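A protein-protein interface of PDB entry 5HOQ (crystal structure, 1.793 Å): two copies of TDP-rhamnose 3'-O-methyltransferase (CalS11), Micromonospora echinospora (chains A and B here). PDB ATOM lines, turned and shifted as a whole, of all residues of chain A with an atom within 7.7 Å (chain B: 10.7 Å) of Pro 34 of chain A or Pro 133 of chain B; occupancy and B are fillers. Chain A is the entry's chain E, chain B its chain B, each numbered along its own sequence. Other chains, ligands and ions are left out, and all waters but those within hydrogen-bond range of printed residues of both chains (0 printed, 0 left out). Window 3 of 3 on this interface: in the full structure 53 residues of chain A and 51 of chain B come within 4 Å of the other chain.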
ATOM      1  N   LEU A  29      -4.624  -7.558  17.967  1.00  0.00           N
ATOM      2  CA  LEU A  29      -5.531  -8.650  17.644  1.00  0.00           C
ATOM      3  C   LEU A  29      -6.213  -9.210  18.880  1.00  0.00           C
ATOM      4  O   LEU A  29      -7.300  -9.790  18.771  1.00  0.00           O
ATOM      5  CB  LEU A  29      -4.752  -9.758  16.924  1.00  0.00           C
ATOM      6  CG  LEU A  29      -4.222  -9.327  15.553  1.00  0.00           C
ATOM      7  CD1 LEU A  29      -3.049 -10.219  15.127  1.00  0.00           C
ATOM      8  CD2 LEU A  29      -5.359  -9.363  14.508  1.00  0.00           C
ATOM      9  N   LEU A  30      -5.585  -9.055  20.049  1.00  0.00           N
ATOM     10  CA  LEU A  30      -6.198  -9.461  21.307  1.00  0.00           C
ATOM     11  C   LEU A  30      -7.344  -8.525  21.687  1.00  0.00           C
ATOM     12  O   LEU A  30      -8.416  -8.975  22.115  1.00  0.00           O
ATOM     13  CB  LEU A  30      -5.136  -9.465  22.407  1.00  0.00           C
ATOM     14  CG  LEU A  30      -5.668  -9.568  23.837  1.00  0.00           C
ATOM     15  CD1 LEU A  30      -6.504 -10.810  24.023  1.00  0.00           C
ATOM     16  CD2 LEU A  30      -4.541  -9.506  24.829  1.00  0.00           C
ATOM     17  N   THR A  31      -7.124  -7.219  21.569  1.00  0.00           N
ATOM     18  CA  THR A  31      -8.097  -6.249  22.056  1.00  0.00           C
ATOM     19  C   THR A  31      -9.182  -5.949  21.031  1.00  0.00           C
ATOM     20  O   THR A  31     -10.182  -5.306  21.367  1.00  0.00           O
ATOM     21  CB  THR A  31      -7.400  -4.939  22.469  1.00  0.00           C
ATOM     22  OG1 THR A  31      -6.669  -4.388  21.371  1.00  0.00           O
ATOM     23  CG2 THR A  31      -6.439  -5.156  23.629  1.00  0.00           C
ATOM     24  N   ASN A  32      -9.005  -6.384  19.787  1.00  0.00           N
ATOM     25  CA  ASN A  32      -9.993  -6.171  18.737  1.00  0.00           C
ATOM     26  C   ASN A  32     -10.334  -7.518  18.118  1.00  0.00           C
ATOM     27  O   ASN A  32     -10.155  -7.742  16.922  1.00  0.00           O
ATOM     28  CB  ASN A  32      -9.481  -5.193  17.685  1.00  0.00           C
ATOM     29  CG  ASN A  32      -9.122  -3.842  18.271  1.00  0.00           C
ATOM     30  OD1 ASN A  32      -9.993  -2.997  18.485  1.00  0.00           O
ATOM     31  ND2 ASN A  32      -7.836  -3.628  18.524  1.00  0.00           N
ATOM     32  N   SER A  33     -10.831  -8.438  18.952  1.00  0.00           N
ATOM     33  CA  SER A  33     -10.918  -9.809  18.461  1.00  0.00           C
ATOM     34  C   SER A  33     -12.349 -10.211  18.149  1.00  0.00           C
ATOM     35  O   SER A  33     -13.262  -9.915  18.927  1.00  0.00           O
ATOM     36  CB  SER A  33     -10.343 -10.802  19.465  1.00  0.00           C
ATOM     37  OG  SER A  33     -10.577 -12.136  19.033  1.00  0.00           O
ATOM     38  N   PRO A  34     -12.575 -10.905  17.030  1.00  0.00           N
ATOM     39  CA  PRO A  34     -13.907 -11.483  16.791  1.00  0.00           C
ATOM     40  C   PRO A  34     -14.246 -12.611  17.747  1.00  0.00           C
ATOM     41  O   PRO A  34     -15.417 -13.002  17.813  1.00  0.00           O
ATOM     42  CB  PRO A  34     -13.830 -11.976  15.334  1.00  0.00           C
ATOM     43  CG  PRO A  34     -12.353 -12.071  15.023  1.00  0.00           C
ATOM     44  CD  PRO A  34     -11.644 -11.119  15.903  1.00  0.00           C
ATOM     45  N   ILE A  35     -13.274 -13.145  18.487  1.00  0.00           N
ATOM     46  CA  ILE A  35     -13.595 -14.161  19.498  1.00  0.00           C
ATOM     47  C   ILE A  35     -14.491 -13.513  20.547  1.00  0.00           C
ATOM     48  O   ILE A  35     -14.226 -12.354  20.940  1.00  0.00           O
ATOM     49  CB  ILE A  35     -12.310 -14.722  20.137  1.00  0.00           C
ATOM     50  CG1 ILE A  35     -11.419 -15.357  19.060  1.00  0.00           C
ATOM     51  CG2 ILE A  35     -12.639 -15.731  21.228  1.00  0.00           C
ATOM     52  CD1 ILE A  35     -10.030 -15.749  19.569  1.00  0.00           C
ATOM     53  N   PRO A  36     -15.585 -14.148  20.987  1.00  0.00           N
ATOM     54  CA  PRO A  36     -16.366 -13.554  22.087  1.00  0.00           C
ATOM     55  C   PRO A  36     -15.460 -13.302  23.280  1.00  0.00           C
ATOM     56  O   PRO A  36     -14.580 -14.110  23.592  1.00  0.00           O
ATOM     57  CB  PRO A  36     -17.429 -14.612  22.393  1.00  0.00           C
ATOM     58  CG  PRO A  36     -17.610 -15.360  21.080  1.00  0.00           C
ATOM     59  CD  PRO A  36     -16.211 -15.379  20.469  1.00  0.00           C
ATOM     60  N   THR A  37     -15.666 -12.163  23.948  1.00  0.00           N
ATOM     61  CA  THR A  37     -14.758 -11.785  25.033  1.00  0.00           C
ATOM     62  C   THR A  37     -14.689 -12.877  26.094  1.00  0.00           C
ATOM     63  O   THR A  37     -13.618 -13.149  26.645  1.00  0.00           O
ATOM     64  CB  THR A  37     -15.204 -10.457  25.636  1.00  0.00           C
ATOM     65  OG1 THR A  37     -15.123  -9.440  24.640  1.00  0.00           O
ATOM     66  CG2 THR A  37     -14.333 -10.060  26.794  1.00  0.00           C
ATOM     67  N   LEU A  40     -11.988 -15.512  25.403  1.00  0.00           N
ATOM     68  CA  LEU A  40     -10.569 -15.194  25.254  1.00  0.00           C
ATOM     69  C   LEU A  40      -9.695 -16.007  26.199  1.00  0.00           C
ATOM     70  O   LEU A  40      -8.611 -16.446  25.803  1.00  0.00           O
ATOM     71  CB  LEU A  40     -10.317 -13.711  25.468  1.00  0.00           C
ATOM     72  CG  LEU A  40     -10.916 -12.821  24.383  1.00  0.00           C
ATOM     73  CD1 LEU A  40     -10.746 -11.362  24.813  1.00  0.00           C
ATOM     74  CD2 LEU A  40     -10.289 -13.085  23.023  1.00  0.00           C
ATOM     75  N   PHE A  47      -2.087 -15.531  21.437  1.00  0.00           N
ATOM     76  CA  PHE A  47      -1.406 -14.255  21.657  1.00  0.00           C
ATOM     77  C   PHE A  47      -0.115 -14.402  22.451  1.00  0.00           C
ATOM     78  O   PHE A  47       0.517 -13.394  22.790  1.00  0.00           O
ATOM     79  CB  PHE A  47      -2.379 -13.279  22.340  1.00  0.00           C
ATOM     80  CG  PHE A  47      -3.756 -13.290  21.709  1.00  0.00           C
ATOM     81  CD1 PHE A  47      -3.976 -12.689  20.482  1.00  0.00           C
ATOM     82  CD2 PHE A  47      -4.812 -13.932  22.328  1.00  0.00           C
ATOM     83  CE1 PHE A  47      -5.237 -12.723  19.879  1.00  0.00           C
ATOM     84  CE2 PHE A  47      -6.072 -13.950  21.747  1.00  0.00           C
ATOM     85  CZ  PHE A  47      -6.278 -13.366  20.519  1.00  0.00           C
ATOM     86  N   ARG B  79     -11.447 -25.065  15.862  1.00  0.00           N
ATOM     87  CA  ARG B  79     -12.213 -24.233  16.808  1.00  0.00           C
ATOM     88  C   ARG B  79     -11.810 -22.783  16.548  1.00  0.00           C
ATOM     89  O   ARG B  79     -11.916 -22.320  15.406  1.00  0.00           O
ATOM     90  CB  ARG B  79     -11.998 -24.720  18.230  1.00  0.00           C
ATOM     91  CG  ARG B  79     -12.164 -26.246  18.447  1.00  0.00           C
ATOM     92  CD  ARG B  79     -13.621 -26.709  18.300  1.00  0.00           C
ATOM     93  NE  ARG B  79     -13.710 -28.175  18.255  1.00  0.00           N
ATOM     94  CZ  ARG B  79     -14.845 -28.865  18.143  1.00  0.00           C
ATOM     95  NH1 ARG B  79     -16.017 -28.234  18.078  1.00  0.00           N
ATOM     96  NH2 ARG B  79     -14.811 -30.191  18.102  1.00  0.00           N
ATOM     97  N   PHE B  80     -11.356 -22.029  17.548  1.00  0.00           N
ATOM     98  CA  PHE B  80     -10.912 -20.659  17.314  1.00  0.00           C
ATOM     99  C   PHE B  80      -9.433 -20.557  16.934  1.00  0.00           C
ATOM    100  O   PHE B  80      -8.968 -19.450  16.641  1.00  0.00           O
ATOM    101  CB  PHE B  80     -11.193 -19.791  18.550  1.00  0.00           C
ATOM    102  CG  PHE B  80     -12.671 -19.470  18.776  1.00  0.00           C
ATOM    103  CD1 PHE B  80     -13.338 -18.572  17.965  1.00  0.00           C
ATOM    104  CD2 PHE B  80     -13.359 -20.044  19.830  1.00  0.00           C
ATOM    105  CE1 PHE B  80     -14.683 -18.257  18.197  1.00  0.00           C
ATOM    106  CE2 PHE B  80     -14.698 -19.736  20.074  1.00  0.00           C
ATOM    107  CZ  PHE B  80     -15.358 -18.849  19.257  1.00  0.00           C
ATOM    108  N   GLY B  81      -8.697 -21.669  16.903  1.00  0.00           N
ATOM    109  CA  GLY B  81      -7.280 -21.684  16.561  1.00  0.00           C
ATOM    110  C   GLY B  81      -6.329 -21.852  17.724  1.00  0.00           C
ATOM    111  O   GLY B  81      -5.111 -21.690  17.529  1.00  0.00           O
ATOM    112  N   ASP B 107     -10.769 -26.622   8.511  1.00  0.00           N
ATOM    113  CA  ASP B 107     -12.043 -26.437   9.198  1.00  0.00           C
ATOM    114  C   ASP B 107     -13.057 -25.908   8.190  1.00  0.00           C
ATOM    115  O   ASP B 107     -12.690 -25.354   7.150  1.00  0.00           O
ATOM    116  CB  ASP B 107     -11.898 -25.477  10.391  1.00  0.00           C
ATOM    117  CG  ASP B 107     -12.949 -25.696  11.460  1.00  0.00           C
ATOM    118  OD1 ASP B 107     -14.129 -25.473  11.171  1.00  0.00           O
ATOM    119  OD2 ASP B 107     -12.612 -26.057  12.606  1.00  0.00           O
ATOM    120  N   THR B 108     -14.342 -26.115   8.492  1.00  0.00           N
ATOM    121  CA  THR B 108     -15.391 -25.448   7.726  1.00  0.00           C
ATOM    122  C   THR B 108     -15.529 -23.985   8.117  1.00  0.00           C
ATOM    123  O   THR B 108     -16.044 -23.184   7.332  1.00  0.00           O
ATOM    124  CB  THR B 108     -16.748 -26.158   7.919  1.00  0.00           C
ATOM    125  OG1 THR B 108     -17.159 -26.064   9.291  1.00  0.00           O
ATOM    126  CG2 THR B 108     -16.663 -27.643   7.526  1.00  0.00           C
ATOM    127  N   PHE B 109     -15.078 -23.620   9.314  1.00  0.00           N
ATOM    128  CA  PHE B 109     -15.184 -22.250   9.818  1.00  0.00           C
ATOM    129  C   PHE B 109     -16.630 -21.744   9.771  1.00  0.00           C
ATOM    130  O   PHE B 109     -16.918 -20.639   9.306  1.00  0.00           O
ATOM    131  CB  PHE B 109     -14.243 -21.322   9.044  1.00  0.00           C
ATOM    132  CG  PHE B 109     -12.791 -21.616   9.288  1.00  0.00           C
ATOM    133  CD1 PHE B 109     -12.209 -21.301  10.500  1.00  0.00           C
ATOM    134  CD2 PHE B 109     -12.019 -22.219   8.316  1.00  0.00           C
ATOM    135  CE1 PHE B 109     -10.882 -21.576  10.740  1.00  0.00           C
ATOM    136  CE2 PHE B 109     -10.675 -22.507   8.554  1.00  0.00           C
ATOM    137  CZ  PHE B 109     -10.112 -22.180   9.771  1.00  0.00           C
ATOM    138  N   THR B 110     -17.542 -22.545  10.307  1.00  0.00           N
ATOM    139  CA  THR B 110     -18.945 -22.152  10.360  1.00  0.00           C
ATOM    140  C   THR B 110     -19.405 -21.928  11.798  1.00  0.00           C
ATOM    141  O   THR B 110     -18.919 -22.576  12.725  1.00  0.00           O
ATOM    142  CB  THR B 110     -19.834 -23.209   9.694  1.00  0.00           C
ATOM    143  OG1 THR B 110     -19.645 -24.474  10.337  1.00  0.00           O
ATOM    144  CG2 THR B 110     -19.489 -23.328   8.208  1.00  0.00           C
ATOM    145  N   VAL B 132     -18.143 -19.629  14.434  1.00  0.00           N
ATOM    146  CA  VAL B 132     -17.248 -18.479  14.382  1.00  0.00           C
ATOM    147  C   VAL B 132     -17.821 -17.398  13.469  1.00  0.00           C
ATOM    148  O   VAL B 132     -18.627 -17.692  12.580  1.00  0.00           O
ATOM    149  CB  VAL B 132     -15.835 -18.880  13.900  1.00  0.00           C
ATOM    150  CG1 VAL B 132     -15.156 -19.791  14.905  1.00  0.00           C
ATOM    151  CG2 VAL B 132     -15.905 -19.550  12.526  1.00  0.00           C
ATOM    152  N   PRO B 133     -17.403 -16.150  13.679  1.00  0.00           N
ATOM    153  CA  PRO B 133     -17.820 -15.074  12.774  1.00  0.00           C
ATOM    154  C   PRO B 133     -17.378 -15.334  11.340  1.00  0.00           C
ATOM    155  O   PRO B 133     -16.445 -16.095  11.072  1.00  0.00           O
ATOM    156  CB  PRO B 133     -17.127 -13.834  13.354  1.00  0.00           C
ATOM    157  CG  PRO B 133     -16.903 -14.163  14.785  1.00  0.00           C
ATOM    158  CD  PRO B 133     -16.641 -15.636  14.831  1.00  0.00           C
ATOM    159  N   GLY B 134     -18.077 -14.695  10.406  1.00  0.00           N
ATOM    160  CA  GLY B 134     -17.624 -14.696   9.027  1.00  0.00           C
ATOM    161  C   GLY B 134     -16.320 -13.927   8.896  1.00  0.00           C
ATOM    162  O   GLY B 134     -16.104 -12.913   9.562  1.00  0.00           O
ATOM    163  N   GLY B 135     -15.438 -14.422   8.027  1.00  0.00           N
ATOM    164  CA  GLY B 135     -14.113 -13.839   7.921  1.00  0.00           C
ATOM    165  C   GLY B 135     -13.212 -14.181   9.086  1.00  0.00           C
ATOM    166  O   GLY B 135     -12.192 -13.519   9.305  1.00  0.00           O
ATOM    167  N   TYR B 136     -13.571 -15.200   9.857  1.00  0.00           N
ATOM    168  CA  TYR B 136     -12.694 -15.631  10.933  1.00  0.00           C
ATOM    169  C   TYR B 136     -11.379 -16.160  10.391  1.00  0.00           C
ATOM    170  O   TYR B 136     -10.325 -15.823  10.962  1.00  0.00           O
ATOM    171  CB  TYR B 136     -13.382 -16.683  11.814  1.00  0.00           C
ATOM    172  CG  TYR B 136     -12.578 -16.858  13.079  1.00  0.00           C
ATOM    173  CD1 TYR B 136     -12.617 -15.894  14.089  1.00  0.00           C
ATOM    174  CD2 TYR B 136     -11.729 -17.944  13.240  1.00  0.00           C
ATOM    175  CE1 TYR B 136     -11.854 -16.015  15.220  1.00  0.00           C
ATOM    176  CE2 TYR B 136     -10.958 -18.082  14.383  1.00  0.00           C
ATOM    177  CZ  TYR B 136     -11.013 -17.122  15.368  1.00  0.00           C
ATOM    178  OH  TYR B 136     -10.235 -17.230  16.504  1.00  0.00           O
ATOM    179  N   PRO B 137     -11.353 -16.953   9.321  1.00  0.00           N
ATOM    180  CA  PRO B 137     -10.056 -17.410   8.794  1.00  0.00           C
ATOM    181  C   PRO B 137      -9.077 -16.280   8.521  1.00  0.00           C
ATOM    182  O   PRO B 137      -7.869 -16.466   8.714  1.00  0.00           O
ATOM    183  CB  PRO B 137     -10.442 -18.143   7.501  1.00  0.00           C
ATOM    184  CG  PRO B 137     -11.854 -18.567   7.694  1.00  0.00           C
ATOM    185  CD  PRO B 137     -12.492 -17.519   8.569  1.00  0.00           C
ATOM    186  N   ALA B 138      -9.561 -15.118   8.054  1.00  0.00           N
ATOM    187  CA  ALA B 138      -8.641 -14.019   7.778  1.00  0.00           C
ATOM    188  C   ALA B 138      -8.039 -13.475   9.066  1.00  0.00           C
ATOM    189  O   ALA B 138      -6.851 -13.125   9.112  1.00  0.00           O
ATOM    190  CB  ALA B 138      -9.356 -12.907   7.012  1.00  0.00           C
ATOM    191  N   TYR B 139      -8.839 -13.407  10.126  1.00  0.00           N
ATOM    192  CA  TYR B 139      -8.318 -12.970  11.422  1.00  0.00           C
ATOM    193  C   TYR B 139      -7.283 -13.952  11.946  1.00  0.00           C
ATOM    194  O   TYR B 139      -6.205 -13.561  12.411  1.00  0.00           O
ATOM    195  CB  TYR B 139      -9.464 -12.835  12.418  1.00  0.00           C
ATOM    196  CG  TYR B 139      -9.038 -12.668  13.873  1.00  0.00           C
ATOM    197  CD1 TYR B 139      -8.626 -11.427  14.362  1.00  0.00           C
ATOM    198  CD2 TYR B 139      -9.071 -13.748  14.759  1.00  0.00           C
ATOM    199  CE1 TYR B 139      -8.250 -11.267  15.698  1.00  0.00           C
ATOM    200  CE2 TYR B 139      -8.704 -13.592  16.096  1.00  0.00           C
ATOM    201  CZ  TYR B 139      -8.291 -12.356  16.551  1.00  0.00           C
ATOM    202  OH  TYR B 139      -7.937 -12.193  17.879  1.00  0.00           O
ATOM    203  N   LEU B 140      -7.613 -15.236  11.918  1.00  0.00           N
ATOM    204  CA  LEU B 140      -6.685 -16.235  12.423  1.00  0.00           C
ATOM    205  C   LEU B 140      -5.392 -16.221  11.624  1.00  0.00           C
ATOM    206  O   LEU B 140      -4.303 -16.355  12.189  1.00  0.00           O
ATOM    207  CB  LEU B 140      -7.363 -17.600  12.393  1.00  0.00           C
ATOM    208  CG  LEU B 140      -6.615 -18.818  12.884  1.00  0.00           C
ATOM    209  CD1 LEU B 140      -6.227 -18.661  14.337  1.00  0.00           C
ATOM    210  CD2 LEU B 140      -7.499 -20.039  12.693  1.00  0.00           C
ATOM    211  N   LYS B 141      -5.486 -16.011  10.314  1.00  0.00           N
ATOM    212  CA  LYS B 141      -4.282 -15.920   9.500  1.00  0.00           C
ATOM    213  C   LYS B 141      -3.440 -14.722   9.914  1.00  0.00           C
ATOM    214  O   LYS B 141      -2.209 -14.789   9.911  1.00  0.00           O
ATOM    215  CB  LYS B 141      -4.665 -15.840   8.016  1.00  0.00           C
ATOM    216  CG  LYS B 141      -3.500 -15.843   7.046  1.00  0.00           C
ATOM    217  CD  LYS B 141      -2.565 -17.041   7.287  1.00  0.00           C
ATOM    218  CE  LYS B 141      -1.538 -17.212   6.171  1.00  0.00           C
ATOM    219  NZ  LYS B 141      -0.209 -17.665   6.693  1.00  0.00           N
ATOM    220  N   GLU B 142      -4.094 -13.613  10.270  1.00  0.00           N
ATOM    221  CA  GLU B 142      -3.376 -12.439  10.755  1.00  0.00           C
ATOM    222  C   GLU B 142      -2.678 -12.727  12.078  1.00  0.00           C
ATOM    223  O   GLU B 142      -1.567 -12.236  12.327  1.00  0.00           O
ATOM    224  CB  GLU B 142      -4.349 -11.261  10.906  1.00  0.00           C
ATOM    225  CG  GLU B 142      -3.841  -9.973  10.338  1.00  0.00           C
ATOM    226  CD  GLU B 142      -4.825  -8.831  10.514  1.00  0.00           C
ATOM    227  OE1 GLU B 142      -6.029  -9.021  10.237  1.00  0.00           O
ATOM    228  OE2 GLU B 142      -4.385  -7.745  10.938  1.00  0.00           O
ATOM    229  N   VAL B 143      -3.317 -13.510  12.948  1.00  0.00           N
ATOM    230  CA  VAL B 143      -2.677 -13.892  14.204  1.00  0.00           C
ATOM    231  C   VAL B 143      -1.429 -14.726  13.925  1.00  0.00           C
ATOM    232  O   VAL B 143      -0.349 -14.492  14.493  1.00  0.00           O
ATOM    233  CB  VAL B 143      -3.682 -14.639  15.097  1.00  0.00           C
ATOM    234  CG1 VAL B 143      -2.984 -15.246  16.293  1.00  0.00           C
ATOM    235  CG2 VAL B 143      -4.794 -13.689  15.559  1.00  0.00           C
ATOM    236  N   GLU B 164     -10.180 -23.851   4.216  1.00  0.00           N
ATOM    237  CA  GLU B 164     -11.607 -23.768   4.532  1.00  0.00           C
ATOM    238  C   GLU B 164     -12.408 -24.736   3.668  1.00  0.00           C
ATOM    239  O   GLU B 164     -12.252 -24.762   2.444  1.00  0.00           O
ATOM    240  CB  GLU B 164     -12.150 -22.346   4.328  1.00  0.00           C
ATOM    241  CG  GLU B 164     -13.648 -22.215   4.702  1.00  0.00           C
ATOM    242  CD  GLU B 164     -14.214 -20.800   4.569  1.00  0.00           C
ATOM    243  OE1 GLU B 164     -15.436 -20.634   4.773  1.00  0.00           O
ATOM    244  OE2 GLU B 164     -13.447 -19.863   4.268  1.00  0.00           O
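Printed residues of chain B within 4 Å of Leu 29 of chain A: Tyr 139 (2.6 Å), Glu 142 (3.8 Å) and Val 143 (3.8 Å). Of chain B, only Tyr 139 comes within 4 Å of Ser 33 of chain A. Printed residues of chain B within 4 Å of Pro 34 of chain A: Pro 133, Tyr 136 and Tyr 139. Of chain B, only Phe 80 (3.8 Å) comes within 4 Å of Pro 36 of chain A. Of the printed residues of chain B, Phe 47 of chain A touches Tyr 139 (3.3 Å). Of the printed residues of chain A, Phe 80 of chain B touches Ile 35 (3.9 Å) and Pro 36 (3.8 Å). Of chain A, only Pro 34 comes within 4 Å of Pro 133 of chain B. Gly 134 of chain B touches none of the printed residues of chain A. Printed residues of chain A within 4 Å of Glu 142 of chain B: Leu 29 (3.8 Å). Of the printed residues of chain A, Val 143 of chain B touches Leu 29 (3.8 Å). The nearest residue of chain B that does not touch Pro 34 of chain A is Phe 80 of chain B (5.3 Å). The nearest printed residue of chain A that does not touch Val 143 of chain B is Phe 47 of chain A (4.4 Å).
Of the 20 printed residues of chain B, 6 touch a printed residue of chain A. Hydrophobic or aromatic side chains of chain B that line the printed part of chain A: Phe 80, Pro 133, Tyr 136, Tyr 139 and Val 143. Of the 11 printed residues of chain A, 6 touch a printed residue of chain B. Hydrophobic or aromatic side chains of chain A that line the printed part of chain B: Leu 29, Pro 34, Ile 35, Pro 36 and Phe 47. Among the printed residues, no Asp or Glu carboxylate lies within 4 Å of a Lys or Arg side-chain nitrogen of the other chain.
No position is printed for both chains.
The backbone carbonyl oxygen (O) of Phe 80 of chain B sits at hydrogen-bond distance from the side-chain hydroxyl (OH) of Tyr 136 of chain B. OG of Ser 33 of chain A lies within hydrogen-bond range of N of Ile 35 of chain A.
Among the printed residues, pairs that only touch across the chains: Leu 29 of chain A with Glu 142 of chain B, Leu 29 of chain A with Val 143 of chain B, Pro 34 of chain A with Pro 133 of chain B, Pro 34 of chain A with Tyr 136 of chain B, Pro 34 of chain A with Tyr 139 of chain B, Ile 35 of chain A with Phe 80 of chain B, Ile 35 of chain A with Tyr 136 of chain B, Pro 36 of chain A with Phe 80 of chain B and Phe 47 of chain A with Tyr 139 of chain B.
The backbone carbonyl oxygen (O) of Leu 29 of chain A lies within hydrogen-bond range of the side-chain hydroxyl (OH) of Tyr 139 of chain B (2.6 Å). The side-chain hydroxyl of Tyr 139 of chain B lies within hydrogen-bond range of the side-chain hydroxyl of Ser 33 of chain A.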
